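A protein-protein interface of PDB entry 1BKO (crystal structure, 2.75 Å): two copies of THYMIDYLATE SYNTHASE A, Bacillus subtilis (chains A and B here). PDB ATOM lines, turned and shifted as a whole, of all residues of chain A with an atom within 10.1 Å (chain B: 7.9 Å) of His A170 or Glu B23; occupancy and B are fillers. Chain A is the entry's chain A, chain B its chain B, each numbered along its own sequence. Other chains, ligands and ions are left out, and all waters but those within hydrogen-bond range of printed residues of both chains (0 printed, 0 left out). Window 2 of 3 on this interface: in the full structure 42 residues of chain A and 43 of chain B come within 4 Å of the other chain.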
ATOM      1  N   LEU A 133      16.403  33.651 -20.970  1.00  0.00           N
ATOM      2  CA  LEU A 133      16.210  32.268 -20.575  1.00  0.00           C
ATOM      3  C   LEU A 133      17.285  31.365 -21.136  1.00  0.00           C
ATOM      4  O   LEU A 133      17.890  30.596 -20.401  1.00  0.00           O
ATOM      5  CB  LEU A 133      14.802  31.771 -20.926  1.00  0.00           C
ATOM      6  CG  LEU A 133      13.766  32.156 -19.856  1.00  0.00           C
ATOM      7  CD1 LEU A 133      12.404  31.533 -20.155  1.00  0.00           C
ATOM      8  CD2 LEU A 133      14.258  31.704 -18.481  1.00  0.00           C
ATOM      9  N   ASN A 136      20.956  33.209 -20.625  1.00  0.00           N
ATOM     10  CA  ASN A 136      21.370  33.425 -19.237  1.00  0.00           C
ATOM     11  C   ASN A 136      20.458  32.677 -18.277  1.00  0.00           C
ATOM     12  O   ASN A 136      19.772  33.271 -17.447  1.00  0.00           O
ATOM     13  CB  ASN A 136      21.371  34.921 -18.877  1.00  0.00           C
ATOM     14  CG  ASN A 136      22.368  35.257 -17.773  1.00  0.00           C
ATOM     15  OD1 ASN A 136      23.120  36.230 -17.880  1.00  0.00           O
ATOM     16  ND2 ASN A 136      22.397  34.442 -16.721  1.00  0.00           N
ATOM     17  N   PRO A 137      20.410  31.350 -18.397  1.00  0.00           N
ATOM     18  CA  PRO A 137      19.557  30.561 -17.508  1.00  0.00           C
ATOM     19  C   PRO A 137      19.884  30.703 -16.011  1.00  0.00           C
ATOM     20  O   PRO A 137      19.028  30.428 -15.162  1.00  0.00           O
ATOM     21  CB  PRO A 137      19.790  29.133 -17.998  1.00  0.00           C
ATOM     22  CG  PRO A 137      21.144  29.176 -18.625  1.00  0.00           C
ATOM     23  CD  PRO A 137      21.114  30.485 -19.357  1.00  0.00           C
ATOM     24  N   SER A 138      21.109  31.124 -15.688  1.00  0.00           N
ATOM     25  CA  SER A 138      21.520  31.265 -14.290  1.00  0.00           C
ATOM     26  C   SER A 138      20.992  32.491 -13.544  1.00  0.00           C
ATOM     27  O   SER A 138      20.922  32.479 -12.307  1.00  0.00           O
ATOM     28  CB  SER A 138      23.047  31.187 -14.161  1.00  0.00           C
ATOM     29  OG  SER A 138      23.696  32.220 -14.885  1.00  0.00           O
ATOM     30  N   TYR A 167      12.671  30.170 -12.842  1.00  0.00           N
ATOM     31  CA  TYR A 167      13.988  29.779 -12.404  1.00  0.00           C
ATOM     32  C   TYR A 167      14.475  28.695 -13.347  1.00  0.00           C
ATOM     33  O   TYR A 167      13.697  27.838 -13.752  1.00  0.00           O
ATOM     34  CB  TYR A 167      13.924  29.222 -10.989  1.00  0.00           C
ATOM     35  CG  TYR A 167      13.235  30.106  -9.970  1.00  0.00           C
ATOM     36  CD1 TYR A 167      13.935  31.095  -9.287  1.00  0.00           C
ATOM     37  CD2 TYR A 167      11.900  29.899  -9.634  1.00  0.00           C
ATOM     38  CE1 TYR A 167      13.323  31.850  -8.280  1.00  0.00           C
ATOM     39  CE2 TYR A 167      11.275  30.648  -8.636  1.00  0.00           C
ATOM     40  CZ  TYR A 167      11.994  31.617  -7.960  1.00  0.00           C
ATOM     41  OH  TYR A 167      11.386  32.341  -6.962  1.00  0.00           O
ATOM     42  N   VAL A 168      15.741  28.764 -13.745  1.00  0.00           N
ATOM     43  CA  VAL A 168      16.309  27.741 -14.619  1.00  0.00           C
ATOM     44  C   VAL A 168      17.405  27.003 -13.880  1.00  0.00           C
ATOM     45  O   VAL A 168      18.413  27.603 -13.494  1.00  0.00           O
ATOM     46  CB  VAL A 168      16.906  28.301 -15.918  1.00  0.00           C
ATOM     47  CG1 VAL A 168      17.589  27.174 -16.680  1.00  0.00           C
ATOM     48  CG2 VAL A 168      15.823  28.903 -16.780  1.00  0.00           C
ATOM     49  N   LYS A 169      17.199  25.709 -13.664  1.00  0.00           N
ATOM     50  CA  LYS A 169      18.190  24.905 -12.964  1.00  0.00           C
ATOM     51  C   LYS A 169      18.288  23.472 -13.473  1.00  0.00           C
ATOM     52  O   LYS A 169      17.420  22.636 -13.204  1.00  0.00           O
ATOM     53  CB  LYS A 169      17.947  24.943 -11.449  1.00  0.00           C
ATOM     54  CG  LYS A 169      18.230  26.312 -10.843  1.00  0.00           C
ATOM     55  CD  LYS A 169      18.138  26.333  -9.329  1.00  0.00           C
ATOM     56  CE  LYS A 169      18.203  27.772  -8.804  1.00  0.00           C
ATOM     57  NZ  LYS A 169      19.456  28.483  -9.198  1.00  0.00           N
ATOM     58  N   HIS A 170      19.390  23.197 -14.171  1.00  0.00           N
ATOM     59  CA  HIS A 170      19.662  21.881 -14.747  1.00  0.00           C
ATOM     60  C   HIS A 170      18.749  21.555 -15.920  1.00  0.00           C
ATOM     61  O   HIS A 170      18.143  20.482 -15.957  1.00  0.00           O
ATOM     62  CB  HIS A 170      19.558  20.777 -13.690  1.00  0.00           C
ATOM     63  CG  HIS A 170      20.630  20.826 -12.646  1.00  0.00           C
ATOM     64  ND1 HIS A 170      21.965  20.645 -12.939  1.00  0.00           N
ATOM     65  CD2 HIS A 170      20.558  21.002 -11.307  1.00  0.00           C
ATOM     66  CE1 HIS A 170      22.671  20.703 -11.824  1.00  0.00           C
ATOM     67  NE2 HIS A 170      21.840  20.918 -10.819  1.00  0.00           N
ATOM     68  N   GLY A 171      18.657  22.477 -16.876  1.00  0.00           N
ATOM     69  CA  GLY A 171      17.825  22.252 -18.047  1.00  0.00           C
ATOM     70  C   GLY A 171      16.329  22.168 -17.787  1.00  0.00           C
ATOM     71  O   GLY A 171      15.570  21.783 -18.674  1.00  0.00           O
ATOM     72  N   LYS A 172      15.910  22.594 -16.596  1.00  0.00           N
ATOM     73  CA  LYS A 172      14.505  22.571 -16.184  1.00  0.00           C
ATOM     74  C   LYS A 172      13.925  23.971 -15.969  1.00  0.00           C
ATOM     75  O   LYS A 172      14.396  24.721 -15.111  1.00  0.00           O
ATOM     76  CB  LYS A 172      14.369  21.803 -14.867  1.00  0.00           C
ATOM     77  CG  LYS A 172      13.463  20.582 -14.905  1.00  0.00           C
ATOM     78  CD  LYS A 172      14.179  19.364 -15.452  1.00  0.00           C
ATOM     79  CE  LYS A 172      13.546  18.079 -14.924  1.00  0.00           C
ATOM     80  NZ  LYS A 172      13.683  17.931 -13.436  1.00  0.00           N
ATOM     81  N   LEU A 173      12.912  24.333 -16.751  1.00  0.00           N
ATOM     82  CA  LEU A 173      12.266  25.633 -16.579  1.00  0.00           C
ATOM     83  C   LEU A 173      11.316  25.466 -15.389  1.00  0.00           C
ATOM     84  O   LEU A 173      10.587  24.470 -15.310  1.00  0.00           O
ATOM     85  CB  LEU A 173      11.479  26.010 -17.834  1.00  0.00           C
ATOM     86  CG  LEU A 173      11.167  27.496 -18.040  1.00  0.00           C
ATOM     87  CD1 LEU A 173      12.459  28.283 -18.238  1.00  0.00           C
ATOM     88  CD2 LEU A 173      10.263  27.684 -19.247  1.00  0.00           C
ATOM     89  N   HIS A 174      11.417  26.367 -14.417  1.00  0.00           N
ATOM     90  CA  HIS A 174      10.573  26.334 -13.220  1.00  0.00           C
ATOM     91  C   HIS A 174       9.756  27.620 -13.143  1.00  0.00           C
ATOM     92  O   HIS A 174      10.301  28.721 -13.309  1.00  0.00           O
ATOM     93  CB  HIS A 174      11.420  26.251 -11.949  1.00  0.00           C
ATOM     94  CG  HIS A 174      12.217  24.989 -11.816  1.00  0.00           C
ATOM     95  ND1 HIS A 174      11.701  23.836 -11.262  1.00  0.00           N
ATOM     96  CD2 HIS A 174      13.516  24.723 -12.090  1.00  0.00           C
ATOM     97  CE1 HIS A 174      12.647  22.916 -11.195  1.00  0.00           C
ATOM     98  NE2 HIS A 174      13.758  23.430 -11.690  1.00  0.00           N
ATOM     99  N   GLY A 207      13.296  25.073 -25.020  1.00  0.00           N
ATOM    100  CA  GLY A 207      13.901  23.759 -25.058  1.00  0.00           C
ATOM    101  C   GLY A 207      14.428  23.320 -23.714  1.00  0.00           C
ATOM    102  O   GLY A 207      15.622  23.059 -23.574  1.00  0.00           O
ATOM    103  N   TYR A 208      13.543  23.232 -22.729  1.00  0.00           N
ATOM    104  CA  TYR A 208      13.919  22.807 -21.388  1.00  0.00           C
ATOM    105  C   TYR A 208      12.893  21.837 -20.863  1.00  0.00           C
ATOM    106  O   TYR A 208      11.699  22.015 -21.060  1.00  0.00           O
ATOM    107  CB  TYR A 208      13.973  23.991 -20.422  1.00  0.00           C
ATOM    108  CG  TYR A 208      15.120  24.956 -20.615  1.00  0.00           C
ATOM    109  CD1 TYR A 208      16.366  24.715 -20.030  1.00  0.00           C
ATOM    110  CD2 TYR A 208      14.942  26.143 -21.324  1.00  0.00           C
ATOM    111  CE1 TYR A 208      17.408  25.642 -20.145  1.00  0.00           C
ATOM    112  CE2 TYR A 208      15.966  27.074 -21.447  1.00  0.00           C
ATOM    113  CZ  TYR A 208      17.199  26.826 -20.855  1.00  0.00           C
ATOM    114  OH  TYR A 208      18.207  27.761 -20.960  1.00  0.00           O
ATOM    115  N   GLU A 209      13.369  20.797 -20.199  1.00  0.00           N
ATOM    116  CA  GLU A 209      12.485  19.807 -19.600  1.00  0.00           C
ATOM    117  C   GLU A 209      11.630  20.494 -18.534  1.00  0.00           C
ATOM    118  O   GLU A 209      12.086  21.416 -17.850  1.00  0.00           O
ATOM    119  CB  GLU A 209      13.301  18.687 -18.956  1.00  0.00           C
ATOM    120  CG  GLU A 209      13.984  17.762 -19.941  1.00  0.00           C
ATOM    121  CD  GLU A 209      13.092  16.619 -20.384  1.00  0.00           C
ATOM    122  OE1 GLU A 209      12.988  15.632 -19.625  1.00  0.00           O
ATOM    123  OE2 GLU A 209      12.502  16.700 -21.483  1.00  0.00           O
ATOM    124  N   LEU A 210      10.398  20.012 -18.394  1.00  0.00           N
ATOM    125  CA  LEU A 210       9.423  20.536 -17.437  1.00  0.00           C
ATOM    126  C   LEU A 210       9.839  20.477 -15.961  1.00  0.00           C
ATOM    127  O   LEU A 210      10.094  19.396 -15.413  1.00  0.00           O
ATOM    128  CB  LEU A 210       8.108  19.792 -17.621  1.00  0.00           C
ATOM    129  CG  LEU A 210       6.911  20.603 -18.108  1.00  0.00           C
ATOM    130  CD1 LEU A 210       7.291  21.515 -19.263  1.00  0.00           C
ATOM    131  CD2 LEU A 210       5.816  19.623 -18.501  1.00  0.00           C
ATOM    132  N   GLY A 211       9.879  21.646 -15.327  1.00  0.00           N
ATOM    133  CA  GLY A 211      10.255  21.729 -13.926  1.00  0.00           C
ATOM    134  C   GLY A 211       9.098  21.685 -12.941  1.00  0.00           C
ATOM    135  O   GLY A 211       8.018  21.187 -13.248  1.00  0.00           O
ATOM    136  N   GLU A 212       9.360  22.154 -11.722  1.00  0.00           N
ATOM    137  CA  GLU A 212       8.354  22.199 -10.658  1.00  0.00           C
ATOM    138  C   GLU A 212       7.432  23.405 -10.908  1.00  0.00           C
ATOM    139  O   GLU A 212       7.867  24.404 -11.505  1.00  0.00           O
ATOM    140  CB  GLU A 212       9.060  22.331  -9.305  1.00  0.00           C
ATOM    141  CG  GLU A 212       8.200  22.022  -8.086  1.00  0.00           C
ATOM    142  CD  GLU A 212       9.003  22.004  -6.780  1.00  0.00           C
ATOM    143  OE1 GLU A 212      10.222  21.706  -6.814  1.00  0.00           O
ATOM    144  OE2 GLU A 212       8.411  22.277  -5.713  1.00  0.00           O
ATOM    145  N   GLY B  18      20.251  20.440  -1.976  1.00  0.00           N
ATOM    146  CA  GLY B  18      20.592  21.624  -2.737  1.00  0.00           C
ATOM    147  C   GLY B  18      20.973  21.338  -4.175  1.00  0.00           C
ATOM    148  O   GLY B  18      21.214  20.192  -4.557  1.00  0.00           O
ATOM    149  N   ILE B  19      21.068  22.401  -4.962  1.00  0.00           N
ATOM    150  CA  ILE B  19      21.415  22.301  -6.364  1.00  0.00           C
ATOM    151  C   ILE B  19      22.475  23.345  -6.682  1.00  0.00           C
ATOM    152  O   ILE B  19      22.296  24.524  -6.399  1.00  0.00           O
ATOM    153  CB  ILE B  19      20.152  22.504  -7.238  1.00  0.00           C
ATOM    154  CG1 ILE B  19      19.465  21.155  -7.452  1.00  0.00           C
ATOM    155  CG2 ILE B  19      20.483  23.216  -8.561  1.00  0.00           C
ATOM    156  CD1 ILE B  19      18.040  21.258  -7.967  1.00  0.00           C
ATOM    157  N   SER B  20      23.572  22.899  -7.283  1.00  0.00           N
ATOM    158  CA  SER B  20      24.673  23.790  -7.635  1.00  0.00           C
ATOM    159  C   SER B  20      24.562  24.400  -9.032  1.00  0.00           C
ATOM    160  O   SER B  20      23.597  24.150  -9.777  1.00  0.00           O
ATOM    161  CB  SER B  20      25.998  23.037  -7.523  1.00  0.00           C
ATOM    162  OG  SER B  20      26.087  22.000  -8.491  1.00  0.00           O
ATOM    163  N   ASP B  21      25.565  25.198  -9.385  1.00  0.00           N
ATOM    164  CA  ASP B  21      25.601  25.828 -10.690  1.00  0.00           C
ATOM    165  C   ASP B  21      27.024  25.841 -11.235  1.00  0.00           C
ATOM    166  O   ASP B  21      27.425  26.774 -11.929  1.00  0.00           O
ATOM    167  CB  ASP B  21      25.008  27.244 -10.641  1.00  0.00           C
ATOM    168  CG  ASP B  21      25.920  28.243  -9.966  1.00  0.00           C
ATOM    169  OD1 ASP B  21      25.959  28.276  -8.711  1.00  0.00           O
ATOM    170  OD2 ASP B  21      26.601  28.993 -10.707  1.00  0.00           O
ATOM    171  N   GLU B  22      27.798  24.821 -10.885  1.00  0.00           N
ATOM    172  CA  GLU B  22      29.168  24.713 -11.371  1.00  0.00           C
ATOM    173  C   GLU B  22      29.149  24.732 -12.894  1.00  0.00           C
ATOM    174  O   GLU B  22      30.035  25.282 -13.546  1.00  0.00           O
ATOM    175  CB  GLU B  22      29.804  23.410 -10.889  1.00  0.00           C
ATOM    176  CG  GLU B  22      30.439  23.470  -9.507  1.00  0.00           C
ATOM    177  CD  GLU B  22      29.425  23.460  -8.377  1.00  0.00           C
ATOM    178  OE1 GLU B  22      28.857  24.533  -8.080  1.00  0.00           O
ATOM    179  OE2 GLU B  22      29.207  22.384  -7.777  1.00  0.00           O
ATOM    180  N   GLU B  23      28.124  24.096 -13.441  1.00  0.00           N
ATOM    181  CA  GLU B  23      27.920  24.002 -14.872  1.00  0.00           C
ATOM    182  C   GLU B  23      27.501  25.339 -15.473  1.00  0.00           C
ATOM    183  O   GLU B  23      26.845  25.371 -16.515  1.00  0.00           O
ATOM    184  CB  GLU B  23      26.843  22.952 -15.155  1.00  0.00           C
ATOM    185  CG  GLU B  23      25.615  23.072 -14.250  1.00  0.00           C
ATOM    186  CD  GLU B  23      24.304  22.853 -14.992  1.00  0.00           C
ATOM    187  OE1 GLU B  23      24.325  22.735 -16.240  1.00  0.00           O
ATOM    188  OE2 GLU B  23      23.244  22.820 -14.327  1.00  0.00           O
ATOM    189  N   PHE B  24      27.853  26.430 -14.799  1.00  0.00           N
ATOM    190  CA  PHE B  24      27.523  27.785 -15.238  1.00  0.00           C
ATOM    191  C   PHE B  24      28.632  28.705 -14.788  1.00  0.00           C
ATOM    192  O   PHE B  24      29.271  28.464 -13.764  1.00  0.00           O
ATOM    193  CB  PHE B  24      26.219  28.299 -14.595  1.00  0.00           C
ATOM    194  CG  PHE B  24      24.981  27.551 -15.011  1.00  0.00           C
ATOM    195  CD1 PHE B  24      24.530  27.594 -16.329  1.00  0.00           C
ATOM    196  CD2 PHE B  24      24.252  26.813 -14.073  1.00  0.00           C
ATOM    197  CE1 PHE B  24      23.371  26.914 -16.708  1.00  0.00           C
ATOM    198  CE2 PHE B  24      23.094  26.129 -14.441  1.00  0.00           C
ATOM    199  CZ  PHE B  24      22.653  26.180 -15.762  1.00  0.00           C
ATOM    200  N   ASP B  25      28.829  29.784 -15.534  1.00  0.00           N
ATOM    201  CA  ASP B  25      29.852  30.776 -15.210  1.00  0.00           C
ATOM    202  C   ASP B  25      29.171  32.081 -14.776  1.00  0.00           C
ATOM    203  O   ASP B  25      28.114  32.060 -14.136  1.00  0.00           O
ATOM    204  CB  ASP B  25      30.756  31.010 -16.440  1.00  0.00           C
ATOM    205  CG  ASP B  25      29.989  31.539 -17.667  1.00  0.00           C
ATOM    206  OD1 ASP B  25      28.783  31.234 -17.828  1.00  0.00           O
ATOM    207  OD2 ASP B  25      30.606  32.266 -18.478  1.00  0.00           O
ATOM    208  N   HIS B  38      30.394  29.370  -6.618  1.00  0.00           N
ATOM    209  CA  HIS B  38      29.047  28.913  -6.919  1.00  0.00           C
ATOM    210  C   HIS B  38      28.183  28.707  -5.686  1.00  0.00           C
ATOM    211  O   HIS B  38      28.625  28.910  -4.554  1.00  0.00           O
ATOM    212  CB  HIS B  38      29.090  27.636  -7.741  1.00  0.00           C
ATOM    213  CG  HIS B  38      30.019  27.706  -8.906  1.00  0.00           C
ATOM    214  ND1 HIS B  38      31.239  27.066  -8.916  1.00  0.00           N
ATOM    215  CD2 HIS B  38      29.925  28.360 -10.088  1.00  0.00           C
ATOM    216  CE1 HIS B  38      31.855  27.321 -10.055  1.00  0.00           C
ATOM    217  NE2 HIS B  38      31.080  28.104 -10.784  1.00  0.00           N
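The side-chain carboxylate (OE2) of Glu B23 is in hydrogen-bond range of a ring nitrogen (ND1) of His A170 (2.9 Å).
OG of Ser B20 sits at hydrogen-bond distance from OE2 of Glu B22 (3.2 Å).
Pro A137 touches Phe B24.
Lys A169 touches Ile B19 (CD to CG2, 3.98 Å).
His A170 touches Ile B19 (NE2 to CG2, 3.5 Å).
Ser B20 touches His A170 (O to NE2, 3.8 Å).
His A170 touches three residues of chain B.
Glu B23 touches just one residue of chain A: His A170.
Ser B20 touches one residue of chain A.
No residue of chain A comes within 4 Å of Glu B22.
Phe B24 touches one residue of chain A.
Printed residues of chain B within 4 Å of Lys A169: Ile B19 (3.98 Å).
Of the printed residues of chain B, Pro A137 touches Phe B24 (3.7 Å).
Of the printed residues of chain A, Ile B19 touches Lys A169 and His A170.
The nearest residue of chain A that does not touch Glu B23 is Lys A169 (5.1 Å).
The nearest printed residue of chain B that does not touch Lys A169 is Glu B23 (5.1 Å).
Of the 18 printed residues of chain A, 3 touch a printed residue of chain B.
Hydrophobic or aromatic side chains of chain A within 4 Å of the printed part of chain B: Pro A137 and His A170.
Along chain A the printed residues that touch a printed residue of chain B span positions 137 to 170.
Of the 9 printed residues of chain B, 4 touch a printed residue of chain A.
Printed residues of chain B that touch a printed residue of chain A: Ile B19, Ser B20, Glu B23 and Phe B24.
Hydrophobic or aromatic side chains of chain B that line the printed part of chain A: Ile B19 and Phe B24.
Among the printed residues, no Asp or Glu carboxylate lies within 4 Å of a Lys or Arg side-chain nitrogen of the other chain.
No position is printed for both chains.
Of the 5 pairs that touch across the chains among the printed residues, none has its exchanged pair printed and touching as well.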
